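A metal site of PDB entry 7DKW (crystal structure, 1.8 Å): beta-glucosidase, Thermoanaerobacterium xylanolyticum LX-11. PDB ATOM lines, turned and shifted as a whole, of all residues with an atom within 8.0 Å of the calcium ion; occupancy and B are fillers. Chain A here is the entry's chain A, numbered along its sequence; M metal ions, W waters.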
ATOM      1  N   LYS A 557     -30.038 -16.382   6.408  1.00  0.00           N
ATOM      2  CA  LYS A 557     -29.231 -15.225   5.992  1.00  0.00           C
ATOM      3  C   LYS A 557     -29.856 -13.869   6.341  1.00  0.00           C
ATOM      4  O   LYS A 557     -29.142 -12.933   6.686  1.00  0.00           O
ATOM      5  CB  LYS A 557     -28.954 -15.275   4.483  1.00  0.00           C
ATOM      6  CG  LYS A 557     -27.967 -14.229   3.954  1.00  0.00           C
ATOM      7  CD  LYS A 557     -26.661 -14.191   4.744  1.00  0.00           C
ATOM      8  CE  LYS A 557     -25.461 -13.805   3.881  1.00  0.00           C
ATOM      9  NZ  LYS A 557     -25.612 -12.474   3.249  1.00  0.00           N
ATOM     10  N   MET A 559     -31.423 -13.109   8.965  1.00  0.00           N
ATOM     11  CA  MET A 559     -31.207 -12.828  10.389  1.00  0.00           C
ATOM     12  C   MET A 559     -29.806 -12.302  10.728  1.00  0.00           C
ATOM     13  O   MET A 559     -29.516 -12.039  11.892  1.00  0.00           O
ATOM     14  CB  MET A 559     -31.530 -14.084  11.212  1.00  0.00           C
ATOM     15  CG  MET A 559     -32.979 -14.539  11.064  1.00  0.00           C
ATOM     16  SD  MET A 559     -33.338 -16.174  11.731  1.00  0.00           S
ATOM     17  CE  MET A 559     -35.073 -16.289  11.299  1.00  0.00           C
ATOM     18  N   ASP A 560     -28.949 -12.155   9.710  1.00  0.00           N
ATOM     19  CA  ASP A 560     -27.717 -11.391   9.842  1.00  0.00           C
ATOM     20  C   ASP A 560     -28.024  -9.897   9.848  1.00  0.00           C
ATOM     21  O   ASP A 560     -28.454  -9.359   8.838  1.00  0.00           O
ATOM     22  CB  ASP A 560     -26.762 -11.692   8.686  1.00  0.00           C
ATOM     23  CG  ASP A 560     -25.483 -10.884   8.740  1.00  0.00           C
ATOM     24  OD1 ASP A 560     -25.162 -10.266   9.795  1.00  0.00           O
ATOM     25  OD2 ASP A 560     -24.770 -10.869   7.738  1.00  0.00           O
ATOM     26  N   LYS A 561     -27.784  -9.242  10.985  1.00  0.00           N
ATOM     27  CA  LYS A 561     -28.214  -7.843  11.223  1.00  0.00           C
ATOM     28  C   LYS A 561     -27.104  -6.771  11.118  1.00  0.00           C
ATOM     29  O   LYS A 561     -27.423  -5.584  11.035  1.00  0.00           O
ATOM     30  CB  LYS A 561     -28.888  -7.740  12.593  1.00  0.00           C
ATOM     31  CG  LYS A 561     -30.144  -8.591  12.707  1.00  0.00           C
ATOM     32  CD  LYS A 561     -30.966  -8.217  13.934  1.00  0.00           C
ATOM     33  CE  LYS A 561     -30.250  -8.561  15.227  1.00  0.00           C
ATOM     34  NZ  LYS A 561     -31.192  -8.533  16.387  1.00  0.00           N
ATOM     35  N   ASP A 562     -25.841  -7.174  11.144  1.00  0.00           N
ATOM     36  CA  ASP A 562     -24.714  -6.249  11.004  1.00  0.00           C
ATOM     37  C   ASP A 562     -23.830  -6.594   9.791  1.00  0.00           C
ATOM     38  O   ASP A 562     -22.661  -6.193   9.724  1.00  0.00           O
ATOM     39  CB  ASP A 562     -23.890  -6.223  12.307  1.00  0.00           C
ATOM     40  CG  ASP A 562     -23.210  -7.549  12.594  1.00  0.00           C
ATOM     41  OD1 ASP A 562     -23.676  -8.602  12.111  1.00  0.00           O
ATOM     42  OD2 ASP A 562     -22.195  -7.534  13.322  1.00  0.00           O
ATOM     43  N   ASN A 563     -24.403  -7.346   8.842  1.00  0.00           N
ATOM     44  CA  ASN A 563     -23.761  -7.695   7.582  1.00  0.00           C
ATOM     45  C   ASN A 563     -22.314  -8.260   7.676  1.00  0.00           C
ATOM     46  O   ASN A 563     -21.472  -8.005   6.814  1.00  0.00           O
ATOM     47  CB  ASN A 563     -23.824  -6.508   6.601  1.00  0.00           C
ATOM     48  CG  ASN A 563     -23.685  -6.943   5.136  1.00  0.00           C
ATOM     49  OD1 ASN A 563     -24.390  -7.837   4.677  1.00  0.00           O
ATOM     50  ND2 ASN A 563     -22.756  -6.323   4.419  1.00  0.00           N
ATOM     51  N   ASP A 564     -22.048  -9.059   8.717  1.00  0.00           N
ATOM     52  CA  ASP A 564     -20.814  -9.861   8.764  1.00  0.00           C
ATOM     53  C   ASP A 564     -20.935 -11.196   8.018  1.00  0.00           C
ATOM     54  O   ASP A 564     -19.975 -11.962   7.978  1.00  0.00           O
ATOM     55  CB  ASP A 564     -20.335 -10.076  10.209  1.00  0.00           C
ATOM     56  CG  ASP A 564     -21.134 -11.150  10.976  1.00  0.00           C
ATOM     57  OD1 ASP A 564     -22.267 -11.499  10.585  1.00  0.00           O
ATOM     58  OD2 ASP A 564     -20.625 -11.613  12.003  1.00  0.00           O
ATOM     59  N   GLY A 565     -22.111 -11.470   7.457  1.00  0.00           N
ATOM     60  CA  GLY A 565     -22.374 -12.680   6.677  1.00  0.00           C
ATOM     61  C   GLY A 565     -22.915 -13.839   7.514  1.00  0.00           C
ATOM     62  O   GLY A 565     -23.109 -14.944   6.998  1.00  0.00           O
ATOM     63  N   ILE A 566     -23.203 -13.586   8.791  1.00  0.00           N
ATOM     64  CA  ILE A 566     -23.564 -14.633   9.752  1.00  0.00           C
ATOM     65  C   ILE A 566     -24.811 -14.225  10.539  1.00  0.00           C
ATOM     66  O   ILE A 566     -24.871 -13.102  11.045  1.00  0.00           O
ATOM     67  CB  ILE A 566     -22.414 -14.898  10.760  1.00  0.00           C
ATOM     68  CG1 ILE A 566     -21.074 -15.119  10.028  1.00  0.00           C
ATOM     69  CG2 ILE A 566     -22.754 -16.096  11.659  1.00  0.00           C
ATOM     70  CD1 ILE A 566     -19.863 -15.179  10.924  1.00  0.00           C
ATOM     71  N   PRO A 567     -25.791 -15.141  10.681  1.00  0.00           N
ATOM     72  CA  PRO A 567     -26.966 -14.879  11.530  1.00  0.00           C
ATOM     73  C   PRO A 567     -26.569 -14.407  12.922  1.00  0.00           C
ATOM     74  O   PRO A 567     -25.593 -14.901  13.476  1.00  0.00           O
ATOM     75  CB  PRO A 567     -27.654 -16.253  11.626  1.00  0.00           C
ATOM     76  CG  PRO A 567     -27.216 -16.997  10.437  1.00  0.00           C
ATOM     77  CD  PRO A 567     -25.889 -16.442   9.985  1.00  0.00           C
ATOM     78  N   ASP A 568     -27.332 -13.454  13.477  1.00  0.00           N
ATOM     79  CA  ASP A 568     -27.093 -12.936  14.821  1.00  0.00           C
ATOM     80  C   ASP A 568     -27.963 -13.620  15.847  1.00  0.00           C
ATOM     81  O   ASP A 568     -29.184 -13.536  15.764  1.00  0.00           O
ATOM     82  CB  ASP A 568     -27.413 -11.432  14.896  1.00  0.00           C
ATOM     83  CG  ASP A 568     -26.340 -10.571  14.300  1.00  0.00           C
ATOM     84  OD1 ASP A 568     -26.043 -10.708  13.088  1.00  0.00           O
ATOM     85  OD2 ASP A 568     -25.790  -9.739  15.052  1.00  0.00           O
ATOM     86  N   ASN A 569     -27.363 -14.267  16.836  1.00  0.00           N
ATOM     87  CA  ASN A 569     -28.134 -14.706  17.990  1.00  0.00           C
ATOM     88  C   ASN A 569     -28.621 -13.434  18.699  1.00  0.00           C
ATOM     89  O   ASN A 569     -27.888 -12.450  18.752  1.00  0.00           O
ATOM     90  CB  ASN A 569     -27.298 -15.599  18.917  1.00  0.00           C
ATOM     91  CG  ASN A 569     -26.994 -16.951  18.296  1.00  0.00           C
ATOM     92  OD1 ASN A 569     -25.986 -17.134  17.596  1.00  0.00           O
ATOM     93  ND2 ASN A 569     -27.910 -17.897  18.489  1.00  0.00           N
ATOM     94  N   GLY A 584     -25.056 -12.213  19.101  1.00  0.00           N
ATOM     95  CA  GLY A 584     -24.106 -11.900  18.053  1.00  0.00           C
ATOM     96  C   GLY A 584     -23.780 -13.164  17.294  1.00  0.00           C
ATOM     97  O   GLY A 584     -24.666 -13.977  17.046  1.00  0.00           O
ATOM     98  N   THR A 585     -22.516 -13.299  16.899  1.00  0.00           N
ATOM     99  CA  THR A 585     -22.019 -14.509  16.255  1.00  0.00           C
ATOM    100  C   THR A 585     -21.631 -15.465  17.403  1.00  0.00           C
ATOM    101  O   THR A 585     -20.860 -15.096  18.273  1.00  0.00           O
ATOM    102  CB  THR A 585     -20.809 -14.207  15.347  1.00  0.00           C
ATOM    103  OG1 THR A 585     -21.209 -13.301  14.305  1.00  0.00           O
ATOM    104  CG2 THR A 585     -20.260 -15.469  14.720  1.00  0.00           C
ATOM    105  N   ASN A 626     -14.977 -13.963   8.669  1.00  0.00           N
ATOM    106  CA  ASN A 626     -15.482 -13.196   9.801  1.00  0.00           C
ATOM    107  C   ASN A 626     -15.662 -14.050  11.070  1.00  0.00           C
ATOM    108  O   ASN A 626     -15.405 -13.564  12.183  1.00  0.00           O
ATOM    109  CB  ASN A 626     -16.762 -12.443   9.434  1.00  0.00           C
ATOM    110  CG  ASN A 626     -16.508 -11.311   8.413  1.00  0.00           C
ATOM    111  OD1 ASN A 626     -15.398 -10.779   8.347  1.00  0.00           O
ATOM    112  ND2 ASN A 626     -17.522 -10.955   7.640  1.00  0.00           N
ATOM    113  N   GLU A 630     -13.721 -12.943  14.396  1.00  0.00           N
ATOM    114  CA  GLU A 630     -14.545 -12.566  15.543  1.00  0.00           C
ATOM    115  C   GLU A 630     -14.329 -13.438  16.773  1.00  0.00           C
ATOM    116  O   GLU A 630     -14.395 -12.934  17.893  1.00  0.00           O
ATOM    117  CB  GLU A 630     -16.025 -12.589  15.163  1.00  0.00           C
ATOM    118  CG  GLU A 630     -16.436 -11.431  14.264  1.00  0.00           C
ATOM    119  CD  GLU A 630     -17.769 -11.664  13.599  1.00  0.00           C
ATOM    120  OE1 GLU A 630     -18.581 -12.460  14.122  1.00  0.00           O
ATOM    121  OE2 GLU A 630     -18.002 -11.049  12.532  1.00  0.00           O
ATOM    122  N   THR A 641     -19.874 -13.235  20.520  1.00  0.00           N
ATOM    123  CA  THR A 641     -19.307 -11.880  20.441  1.00  0.00           C
ATOM    124  C   THR A 641     -19.885 -10.848  21.436  1.00  0.00           C
ATOM    125  O   THR A 641     -19.195  -9.896  21.769  1.00  0.00           O
ATOM    126  CB  THR A 641     -19.410 -11.312  19.012  1.00  0.00           C
ATOM    127  OG1 THR A 641     -20.739 -11.458  18.523  1.00  0.00           O
ATOM    128  CG2 THR A 641     -18.462 -12.038  18.073  1.00  0.00           C
ATOM    129  N   GLU A 642     -21.115 -11.050  21.921  1.00  0.00           N
ATOM    130  CA  GLU A 642     -21.826  -9.989  22.679  1.00  0.00           C
ATOM    131  C   GLU A 642     -22.381 -10.322  24.079  1.00  0.00           C
ATOM    132  O   GLU A 642     -22.919  -9.430  24.746  1.00  0.00           O
ATOM    133  CB  GLU A 642     -22.935  -9.403  21.800  1.00  0.00           C
ATOM    134  CG  GLU A 642     -22.398  -8.635  20.596  1.00  0.00           C
ATOM    135  CD  GLU A 642     -23.448  -8.337  19.543  1.00  0.00           C
ATOM    136  OE1 GLU A 642     -24.539  -7.854  19.912  1.00  0.00           O
ATOM    137  OE2 GLU A 642     -23.185  -8.605  18.350  1.00  0.00           O
HETATM  138 CA    CA M   1     -24.124 -10.988  11.920  1.00  0.00          CA
HETATM  139  O   HOH W   1     -23.658 -12.724  13.618  1.00  0.00           O
HETATM  140  O   HOH W   2     -22.417 -10.290  14.069  1.00  0.00           O
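Of the 18 residues printed, 5 come within 4 Å of the calcium ion. The nearest printed residue that does not touch the calcium ion is Lys 561 (4.2 Å).
The backbone NH (N) of Lys 561 sits close to the side-chain carboxylate (OD1) of Asp 568 (3.1 Å). The backbone carbonyl oxygen (O) of Met 559 is in hydrogen-bond range of the backbone NH (N) of Asp 568, 3.0 Å away. The side-chain carboxylate of Asp 564 is in hydrogen-bond range of the side-chain hydroxyl of Thr 585, at 2.9 Å. OD2 of Asp 564 sits close to OE2 of Glu 630 (2.7 Å). O of Asp 564 is in hydrogen-bond range of ND2 of Asn 626 (2.7 Å). OD1 of Asp 560 lies close to N of Asn 563 (3.2 Å). The side-chain carboxylate (OD2) of Asp 560 is in hydrogen-bond range of the backbone NH (N) of Gly 565.
Water W2 lies within hydrogen-bond range of the side-chain carboxylate of Asp 562, the side-chain carboxylate of Asp 564 and the side-chain hydroxyl of Thr 585. Water W1 bridges OG1 of Thr 585 (2.6 Å) and O of Pro 567 (2.9 Å).
The calcium ion is bound by OD1 of Asp 568 (2.3 Å), OD1 of Asp 564 (2.3 Å), O of Ile 566 (2.4 Å), OD1 of Asp 562 (2.4 Å), water W1 (2.5 Å), OD1 of Asp 560 (2.5 Å) and water W2 (2.8 Å). The calcium ion has seven donor atoms within binding distance.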
